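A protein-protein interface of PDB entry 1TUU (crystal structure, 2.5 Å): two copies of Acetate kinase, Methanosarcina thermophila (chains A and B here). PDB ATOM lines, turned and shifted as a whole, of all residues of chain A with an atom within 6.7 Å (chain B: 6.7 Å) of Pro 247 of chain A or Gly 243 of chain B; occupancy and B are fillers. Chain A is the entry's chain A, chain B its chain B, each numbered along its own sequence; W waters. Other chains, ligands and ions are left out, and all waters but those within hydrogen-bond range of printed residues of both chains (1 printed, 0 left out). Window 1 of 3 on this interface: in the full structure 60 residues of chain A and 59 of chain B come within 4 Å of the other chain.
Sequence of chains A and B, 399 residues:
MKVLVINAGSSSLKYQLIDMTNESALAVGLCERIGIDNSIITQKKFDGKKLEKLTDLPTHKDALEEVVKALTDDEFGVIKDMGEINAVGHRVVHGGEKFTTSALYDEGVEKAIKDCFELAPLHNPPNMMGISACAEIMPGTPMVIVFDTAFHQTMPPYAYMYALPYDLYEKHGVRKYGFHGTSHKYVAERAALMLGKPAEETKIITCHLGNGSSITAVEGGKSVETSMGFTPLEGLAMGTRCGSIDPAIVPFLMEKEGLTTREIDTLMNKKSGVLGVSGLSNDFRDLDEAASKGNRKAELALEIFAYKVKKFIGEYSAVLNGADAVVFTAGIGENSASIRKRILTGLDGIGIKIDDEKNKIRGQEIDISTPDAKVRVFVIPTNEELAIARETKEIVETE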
ATOM      1  N   ALA A 163      14.142 -11.432 -26.460  1.00  0.00           N
ATOM      2  CA  ALA A 163      15.118 -10.392 -26.198  1.00  0.00           C
ATOM      3  C   ALA A 163      16.372 -11.006 -25.586  1.00  0.00           C
ATOM      4  O   ALA A 163      16.768 -10.657 -24.474  1.00  0.00           O
ATOM      5  CB  ALA A 163      14.527  -9.336 -25.265  1.00  0.00           C
ATOM      6  N   SER A 244       4.690 -18.682 -18.157  1.00  0.00           N
ATOM      7  CA  SER A 244       5.641 -17.589 -18.027  1.00  0.00           C
ATOM      8  C   SER A 244       5.884 -17.142 -16.592  1.00  0.00           C
ATOM      9  O   SER A 244       5.130 -16.356 -16.039  1.00  0.00           O
ATOM     10  CB  SER A 244       5.174 -16.399 -18.866  1.00  0.00           C
ATOM     11  OG  SER A 244       5.019 -16.778 -20.220  1.00  0.00           O
ATOM     12  N   ILE A 245       6.940 -17.671 -15.987  1.00  0.00           N
ATOM     13  CA  ILE A 245       7.325 -17.302 -14.628  1.00  0.00           C
ATOM     14  C   ILE A 245       8.605 -16.493 -14.781  1.00  0.00           C
ATOM     15  O   ILE A 245       9.164 -16.406 -15.881  1.00  0.00           O
ATOM     16  CB  ILE A 245       7.651 -18.540 -13.743  1.00  0.00           C
ATOM     17  CG1 ILE A 245       8.818 -19.338 -14.351  1.00  0.00           C
ATOM     18  CG2 ILE A 245       6.424 -19.426 -13.570  1.00  0.00           C
ATOM     19  CD1 ILE A 245       9.194 -20.611 -13.568  1.00  0.00           C
ATOM     20  N   ASP A 246       9.081 -15.904 -13.691  1.00  0.00           N
ATOM     21  CA  ASP A 246      10.336 -15.154 -13.735  1.00  0.00           C
ATOM     22  C   ASP A 246      11.380 -16.211 -14.058  1.00  0.00           C
ATOM     23  O   ASP A 246      11.485 -17.195 -13.359  1.00  0.00           O
ATOM     24  CB  ASP A 246      10.637 -14.542 -12.367  1.00  0.00           C
ATOM     25  CG  ASP A 246      11.945 -13.767 -12.346  1.00  0.00           C
ATOM     26  OD1 ASP A 246      12.689 -13.836 -13.351  1.00  0.00           O
ATOM     27  OD2 ASP A 246      12.221 -13.085 -11.328  1.00  0.00           O
ATOM     28  N   PRO A 247      12.161 -16.024 -15.129  1.00  0.00           N
ATOM     29  CA  PRO A 247      13.177 -17.025 -15.487  1.00  0.00           C
ATOM     30  C   PRO A 247      14.281 -17.169 -14.448  1.00  0.00           C
ATOM     31  O   PRO A 247      14.837 -18.249 -14.261  1.00  0.00           O
ATOM     32  CB  PRO A 247      13.713 -16.516 -16.826  1.00  0.00           C
ATOM     33  CG  PRO A 247      12.600 -15.667 -17.369  1.00  0.00           C
ATOM     34  CD  PRO A 247      12.135 -14.938 -16.124  1.00  0.00           C
ATOM     35  N   ALA A 248      14.599 -16.074 -13.775  1.00  0.00           N
ATOM     36  CA  ALA A 248      15.620 -16.106 -12.752  1.00  0.00           C
ATOM     37  C   ALA A 248      15.316 -17.192 -11.716  1.00  0.00           C
ATOM     38  O   ALA A 248      16.223 -17.636 -11.008  1.00  0.00           O
ATOM     39  CB  ALA A 248      15.723 -14.731 -12.076  1.00  0.00           C
ATOM     40  N   ILE A 249      14.055 -17.629 -11.635  1.00  0.00           N
ATOM     41  CA  ILE A 249      13.658 -18.670 -10.678  1.00  0.00           C
ATOM     42  C   ILE A 249      14.297 -20.018 -10.997  1.00  0.00           C
ATOM     43  O   ILE A 249      14.544 -20.831 -10.107  1.00  0.00           O
ATOM     44  CB  ILE A 249      12.125 -18.853 -10.630  1.00  0.00           C
ATOM     45  CG1 ILE A 249      11.485 -17.571 -10.119  1.00  0.00           C
ATOM     46  CG2 ILE A 249      11.741 -19.992  -9.695  1.00  0.00           C
ATOM     47  CD1 ILE A 249       9.989 -17.665  -9.991  1.00  0.00           C
ATOM     48  N   VAL A 250      14.556 -20.255 -12.276  1.00  0.00           N
ATOM     49  CA  VAL A 250      15.190 -21.490 -12.703  1.00  0.00           C
ATOM     50  C   VAL A 250      16.560 -21.645 -12.037  1.00  0.00           C
ATOM     51  O   VAL A 250      16.772 -22.564 -11.234  1.00  0.00           O
ATOM     52  CB  VAL A 250      15.367 -21.503 -14.212  1.00  0.00           C
ATOM     53  CG1 VAL A 250      15.906 -22.843 -14.652  1.00  0.00           C
ATOM     54  CG2 VAL A 250      14.042 -21.205 -14.884  1.00  0.00           C
ATOM     55  N   PRO A 251      17.507 -20.736 -12.346  1.00  0.00           N
ATOM     56  CA  PRO A 251      18.833 -20.854 -11.728  1.00  0.00           C
ATOM     57  C   PRO A 251      18.734 -20.842 -10.200  1.00  0.00           C
ATOM     58  O   PRO A 251      19.462 -21.568  -9.513  1.00  0.00           O
ATOM     59  CB  PRO A 251      19.581 -19.645 -12.284  1.00  0.00           C
ATOM     60  CG  PRO A 251      18.511 -18.632 -12.408  1.00  0.00           C
ATOM     61  CD  PRO A 251      17.360 -19.428 -13.010  1.00  0.00           C
ATOM     62  N   PHE A 252      17.824 -20.020  -9.682  1.00  0.00           N
ATOM     63  CA  PHE A 252      17.616 -19.920  -8.243  1.00  0.00           C
ATOM     64  C   PHE A 252      17.243 -21.274  -7.648  1.00  0.00           C
ATOM     65  O   PHE A 252      17.912 -21.779  -6.740  1.00  0.00           O
ATOM     66  CB  PHE A 252      16.491 -18.938  -7.941  1.00  0.00           C
ATOM     67  CG  PHE A 252      16.064 -18.929  -6.505  1.00  0.00           C
ATOM     68  CD1 PHE A 252      16.814 -18.257  -5.547  1.00  0.00           C
ATOM     69  CD2 PHE A 252      14.886 -19.564  -6.113  1.00  0.00           C
ATOM     70  CE1 PHE A 252      16.398 -18.207  -4.218  1.00  0.00           C
ATOM     71  CE2 PHE A 252      14.461 -19.520  -4.787  1.00  0.00           C
ATOM     72  CZ  PHE A 252      15.217 -18.839  -3.839  1.00  0.00           C
ATOM     73  N   THR B 231      12.245 -11.400  -9.178  1.00  0.00           N
ATOM     74  CA  THR B 231      13.459 -10.619  -9.395  1.00  0.00           C
ATOM     75  C   THR B 231      13.181  -9.533 -10.439  1.00  0.00           C
ATOM     76  O   THR B 231      12.104  -9.505 -11.051  1.00  0.00           O
ATOM     77  CB  THR B 231      14.655 -11.484  -9.908  1.00  0.00           C
ATOM     78  OG1 THR B 231      14.470 -11.803 -11.292  1.00  0.00           O
ATOM     79  CG2 THR B 231      14.780 -12.747  -9.104  1.00  0.00           C
ATOM     80  N   PRO B 232      14.146  -8.623 -10.651  1.00  0.00           N
ATOM     81  CA  PRO B 232      13.943  -7.564 -11.640  1.00  0.00           C
ATOM     82  C   PRO B 232      14.021  -8.110 -13.062  1.00  0.00           C
ATOM     83  O   PRO B 232      13.845  -7.374 -14.039  1.00  0.00           O
ATOM     84  CB  PRO B 232      15.069  -6.587 -11.333  1.00  0.00           C
ATOM     85  CG  PRO B 232      15.288  -6.779  -9.845  1.00  0.00           C
ATOM     86  CD  PRO B 232      15.260  -8.284  -9.750  1.00  0.00           C
ATOM     87  N   LEU B 233      14.277  -9.410 -13.180  1.00  0.00           N
ATOM     88  CA  LEU B 233      14.401 -10.034 -14.498  1.00  0.00           C
ATOM     89  C   LEU B 233      13.076 -10.209 -15.234  1.00  0.00           C
ATOM     90  O   LEU B 233      13.007 -10.052 -16.447  1.00  0.00           O
ATOM     91  CB  LEU B 233      15.089 -11.393 -14.388  1.00  0.00           C
ATOM     92  CG  LEU B 233      15.277 -12.107 -15.731  1.00  0.00           C
ATOM     93  CD1 LEU B 233      16.231 -11.333 -16.610  1.00  0.00           C
ATOM     94  CD2 LEU B 233      15.808 -13.503 -15.478  1.00  0.00           C
ATOM     95  N   GLU B 234      12.023 -10.532 -14.503  1.00  0.00           N
ATOM     96  CA  GLU B 234      10.736 -10.740 -15.133  1.00  0.00           C
ATOM     97  C   GLU B 234      10.064  -9.480 -15.660  1.00  0.00           C
ATOM     98  O   GLU B 234      10.204  -8.398 -15.099  1.00  0.00           O
ATOM     99  CB  GLU B 234       9.796 -11.446 -14.170  1.00  0.00           C
ATOM    100  CG  GLU B 234       8.416 -11.682 -14.722  1.00  0.00           C
ATOM    101  CD  GLU B 234       7.565 -12.412 -13.738  1.00  0.00           C
ATOM    102  OE1 GLU B 234       7.943 -12.459 -12.549  1.00  0.00           O
ATOM    103  OE2 GLU B 234       6.516 -12.936 -14.140  1.00  0.00           O
ATOM    104  N   GLY B 235       9.329  -9.639 -16.751  1.00  0.00           N
ATOM    105  CA  GLY B 235       8.630  -8.513 -17.313  1.00  0.00           C
ATOM    106  C   GLY B 235       9.066  -8.167 -18.720  1.00  0.00           C
ATOM    107  O   GLY B 235       9.257  -9.038 -19.566  1.00  0.00           O
ATOM    108  N   LEU B 236       9.254  -6.878 -18.962  1.00  0.00           N
ATOM    109  CA  LEU B 236       9.650  -6.398 -20.270  1.00  0.00           C
ATOM    110  C   LEU B 236      11.110  -6.661 -20.622  1.00  0.00           C
ATOM    111  O   LEU B 236      11.915  -7.012 -19.765  1.00  0.00           O
ATOM    112  CB  LEU B 236       9.404  -4.894 -20.359  1.00  0.00           C
ATOM    113  CG  LEU B 236       8.021  -4.384 -20.012  1.00  0.00           C
ATOM    114  CD1 LEU B 236       8.148  -2.962 -19.470  1.00  0.00           C
ATOM    115  CD2 LEU B 236       7.146  -4.443 -21.239  1.00  0.00           C
ATOM    116  N   ALA B 237      11.442  -6.485 -21.897  1.00  0.00           N
ATOM    117  CA  ALA B 237      12.814  -6.635 -22.304  1.00  0.00           C
ATOM    118  C   ALA B 237      13.345  -5.279 -21.849  1.00  0.00           C
ATOM    119  O   ALA B 237      12.628  -4.277 -21.926  1.00  0.00           O
ATOM    120  CB  ALA B 237      12.918  -6.778 -23.806  1.00  0.00           C
ATOM    121  N   MET B 238      14.579  -5.244 -21.358  1.00  0.00           N
ATOM    122  CA  MET B 238      15.158  -3.998 -20.868  1.00  0.00           C
ATOM    123  C   MET B 238      16.527  -3.716 -21.506  1.00  0.00           C
ATOM    124  O   MET B 238      16.849  -4.303 -22.528  1.00  0.00           O
ATOM    125  CB  MET B 238      15.245  -4.072 -19.336  1.00  0.00           C
ATOM    126  CG  MET B 238      13.931  -4.481 -18.695  1.00  0.00           C
ATOM    127  SD  MET B 238      14.027  -4.835 -16.971  1.00  0.00           S
ATOM    128  CE  MET B 238      13.016  -6.284 -16.914  1.00  0.00           C
ATOM    129  N   ARG B 241      18.345  -6.926 -19.926  1.00  0.00           N
ATOM    130  CA  ARG B 241      17.530  -8.046 -19.466  1.00  0.00           C
ATOM    131  C   ARG B 241      16.582  -8.573 -20.545  1.00  0.00           C
ATOM    132  O   ARG B 241      16.014  -7.800 -21.307  1.00  0.00           O
ATOM    133  CB  ARG B 241      16.711  -7.618 -18.246  1.00  0.00           C
ATOM    134  CG  ARG B 241      17.508  -7.062 -17.061  1.00  0.00           C
ATOM    135  CD  ARG B 241      16.815  -7.536 -15.781  1.00  0.00           C
ATOM    136  NE  ARG B 241      17.402  -7.031 -14.548  1.00  0.00           N
ATOM    137  CZ  ARG B 241      17.282  -5.779 -14.123  1.00  0.00           C
ATOM    138  NH1 ARG B 241      16.596  -4.896 -14.837  1.00  0.00           N
ATOM    139  NH2 ARG B 241      17.825  -5.418 -12.968  1.00  0.00           N
ATOM    140  N   CYS B 242      16.397  -9.891 -20.577  1.00  0.00           N
ATOM    141  CA  CYS B 242      15.519 -10.543 -21.545  1.00  0.00           C
ATOM    142  C   CYS B 242      14.042 -10.448 -21.157  1.00  0.00           C
ATOM    143  O   CYS B 242      13.169 -10.402 -22.025  1.00  0.00           O
ATOM    144  CB  CYS B 242      15.891 -12.011 -21.666  1.00  0.00           C
ATOM    145  SG  CYS B 242      15.613 -12.938 -20.186  1.00  0.00           S
ATOM    146  N   GLY B 243      13.768 -10.443 -19.855  1.00  0.00           N
ATOM    147  CA  GLY B 243      12.393 -10.372 -19.385  1.00  0.00           C
ATOM    148  C   GLY B 243      11.705 -11.728 -19.388  1.00  0.00           C
ATOM    149  O   GLY B 243      12.375 -12.761 -19.368  1.00  0.00           O
ATOM    150  N   SER B 244      10.375 -11.747 -19.419  1.00  0.00           N
ATOM    151  CA  SER B 244       9.654 -13.019 -19.410  1.00  0.00           C
ATOM    152  C   SER B 244       9.728 -13.775 -20.718  1.00  0.00           C
ATOM    153  O   SER B 244       9.022 -13.464 -21.669  1.00  0.00           O
ATOM    154  CB  SER B 244       8.180 -12.815 -19.042  1.00  0.00           C
ATOM    155  OG  SER B 244       8.039 -12.373 -17.704  1.00  0.00           O
ATOM    156  N   ILE B 245      10.590 -14.783 -20.749  1.00  0.00           N
ATOM    157  CA  ILE B 245      10.755 -15.638 -21.916  1.00  0.00           C
ATOM    158  C   ILE B 245      10.224 -17.003 -21.523  1.00  0.00           C
ATOM    159  O   ILE B 245       9.758 -17.198 -20.400  1.00  0.00           O
ATOM    160  CB  ILE B 245      12.243 -15.815 -22.312  1.00  0.00           C
ATOM    161  CG1 ILE B 245      13.050 -16.369 -21.138  1.00  0.00           C
ATOM    162  CG2 ILE B 245      12.836 -14.506 -22.757  1.00  0.00           C
ATOM    163  CD1 ILE B 245      14.482 -16.733 -21.488  1.00  0.00           C
ATOM    164  N   ASP B 246      10.292 -17.947 -22.447  1.00  0.00           N
ATOM    165  CA  ASP B 246       9.839 -19.303 -22.175  1.00  0.00           C
ATOM    166  C   ASP B 246      10.831 -19.860 -21.157  1.00  0.00           C
ATOM    167  O   ASP B 246      12.030 -19.906 -21.415  1.00  0.00           O
ATOM    168  CB  ASP B 246       9.886 -20.128 -23.469  1.00  0.00           C
ATOM    169  CG  ASP B 246       9.581 -21.597 -23.245  1.00  0.00           C
ATOM    170  OD1 ASP B 246       9.540 -22.028 -22.069  1.00  0.00           O
ATOM    171  OD2 ASP B 246       9.406 -22.334 -24.251  1.00  0.00           O
ATOM    172  N   PRO B 247      10.350 -20.275 -19.975  1.00  0.00           N
ATOM    173  CA  PRO B 247      11.271 -20.820 -18.964  1.00  0.00           C
ATOM    174  C   PRO B 247      12.105 -22.005 -19.458  1.00  0.00           C
ATOM    175  O   PRO B 247      13.216 -22.209 -18.993  1.00  0.00           O
ATOM    176  CB  PRO B 247      10.331 -21.236 -17.829  1.00  0.00           C
ATOM    177  CG  PRO B 247       9.188 -20.293 -17.958  1.00  0.00           C
ATOM    178  CD  PRO B 247       8.971 -20.208 -19.451  1.00  0.00           C
ATOM    179  N   VAL B 250      15.852 -21.604 -20.466  1.00  0.00           N
ATOM    180  CA  VAL B 250      16.946 -21.574 -19.490  1.00  0.00           C
ATOM    181  C   VAL B 250      17.674 -22.905 -19.385  1.00  0.00           C
ATOM    182  O   VAL B 250      18.873 -22.975 -19.625  1.00  0.00           O
ATOM    183  CB  VAL B 250      16.457 -21.186 -18.077  1.00  0.00           C
ATOM    184  CG1 VAL B 250      17.643 -21.059 -17.134  1.00  0.00           C
ATOM    185  CG2 VAL B 250      15.669 -19.884 -18.131  1.00  0.00           C
ATOM    186  N   MET B 268      21.124 -13.652 -18.980  1.00  0.00           N
ATOM    187  CA  MET B 268      19.780 -13.081 -19.054  1.00  0.00           C
ATOM    188  C   MET B 268      19.657 -11.660 -18.482  1.00  0.00           C
ATOM    189  O   MET B 268      18.847 -10.857 -18.955  1.00  0.00           O
ATOM    190  CB  MET B 268      18.775 -14.002 -18.338  1.00  0.00           C
ATOM    191  CG  MET B 268      18.864 -15.459 -18.733  1.00  0.00           C
ATOM    192  SD  MET B 268      17.368 -16.372 -18.257  1.00  0.00           S
ATOM    193  CE  MET B 268      17.648 -16.635 -16.500  1.00  0.00           C
ATOM    194  N   SER B 272      21.687  -9.812 -22.321  1.00  0.00           N
ATOM    195  CA  SER B 272      20.451  -9.862 -23.101  1.00  0.00           C
ATOM    196  C   SER B 272      19.847  -8.477 -23.344  1.00  0.00           C
ATOM    197  O   SER B 272      20.572  -7.509 -23.507  1.00  0.00           O
ATOM    198  CB  SER B 272      19.444 -10.775 -22.399  1.00  0.00           C
ATOM    199  OG  SER B 272      19.853 -12.135 -22.477  1.00  0.00           O
ATOM    200  N   GLY B 273      18.521  -8.395 -23.375  1.00  0.00           N
ATOM    201  CA  GLY B 273      17.850  -7.124 -23.585  1.00  0.00           C
ATOM    202  C   GLY B 273      18.039  -6.517 -24.964  1.00  0.00           C
ATOM    203  O   GLY B 273      18.262  -7.226 -25.935  1.00  0.00           O
ATOM    204  N   LYS B 308       6.479  -5.034 -26.529  1.00  0.00           N
ATOM    205  CA  LYS B 308       6.271  -5.605 -25.216  1.00  0.00           C
ATOM    206  C   LYS B 308       5.544  -4.629 -24.315  1.00  0.00           C
ATOM    207  O   LYS B 308       4.535  -4.973 -23.701  1.00  0.00           O
ATOM    208  CB  LYS B 308       7.600  -6.040 -24.620  1.00  0.00           C
ATOM    209  CG  LYS B 308       8.143  -7.261 -25.333  1.00  0.00           C
ATOM    210  CD  LYS B 308       9.425  -7.773 -24.736  1.00  0.00           C
ATOM    211  CE  LYS B 308       9.630  -9.206 -25.159  1.00  0.00           C
ATOM    212  NZ  LYS B 308       8.464 -10.043 -24.755  1.00  0.00           N
HETATM  213  O   HOH W   1      12.414 -11.430 -24.577  1.00  0.00           O
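Water W1 lies within hydrogen-bond range of the backbone NH of Ala 163 of chain A and the backbone carbonyl oxygen of Cys 242 of chain B.
N of Ala 248 of chain A sits at hydrogen-bond distance from OD1 of Asp 246 of chain A (3.0 Å).
OG1 of Thr 231 of chain B sits close to N of Leu 233 of chain B, 3.1 Å away.
O of Arg 241 of chain B sits close to N of Gly 273 of chain B (3.3 Å).
O of Met 268 of chain B sits at hydrogen-bond distance from N of Cys 242 of chain B, at 3.1 Å.
Ile 245 of chain A touches Pro 247 of chain B, and with the chains exchanged Pro 247 of chain A touches Ile 245 of chain B.
Val 250 of chain B touches its own counterpart, Val 250 of chain A.
5 positions are printed for both chains.
Of the 15 pairs that touch across the chains among the printed residues, 3 have their exchanged pair printed and touching as well.
Printed residues of chain B within 4 Å of Ala 163 of chain A: Ala 237, Cys 242, Ser 272 and Gly 273.
Of chain B, only Leu 233, Gly 243, Ile 245 and Met 268 come within 4 Å of Pro 247 of chain A.
Of the printed residues of chain A, Thr 231 of chain B touches Asp 246 and Ala 248.
Met 238 of chain B touches none of the printed residues of chain A.
Ser 244 of chain B touches none of the printed residues of chain A.
The nearest residue of chain B that does not touch Pro 247 of chain A is Val 250 of chain B (4.1 Å).
The nearest printed residue of chain A that does not touch Glu 234 of chain B is Ser 244 of chain A (4.2 Å).
Ala 163 of chain A touches Ala 237 of chain B (CB to CB, 3.4 Å).
Ala 163 of chain A touches Cys 242 of chain B (O to CA, 3.2 Å).
Ser 272 of chain B touches Ala 163 of chain A (CB to O, 3.4 Å).
CG1 of Ile 245 of chain A touches CG of Pro 247 of chain B, at 3.7 Å.
Leu 233 of chain B touches Asp 246 of chain A (CB to OD1, 3.6 Å).
CG of Pro 247 of chain A touches O of Gly 243 of chain B, at 3.5 Å.
CG of Pro 247 of chain A touches CG1 of Ile 245 of chain B, 3.9 Å away.
Pro 247 of chain A touches Met 268 of chain B (CB to SD, 3.9 Å).
Ala 248 of chain A touches Thr 231 of chain B (CB to OG1, 3.3 Å).
CG1 of Val 250 of chain A touches CG1 of Val 250 of chain B, 3.5 Å away.
Hydrophobic or aromatic side chains of chain A that line the printed part of chain B: Ala 163, Ile 245, Pro 247, Ala 248 and Val 250.
Along chain B the printed residues that touch a printed residue of chain A span positions 231 to 273.
N of Gly 273 of chain B sits at hydrogen-bond distance from O of Ala 163 of chain A (3.1 Å).
The side-chain carboxylate of Asp 246 of chain A sits at hydrogen-bond distance from the side-chain hydroxyl of Thr 231 of chain B (2.6 Å).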
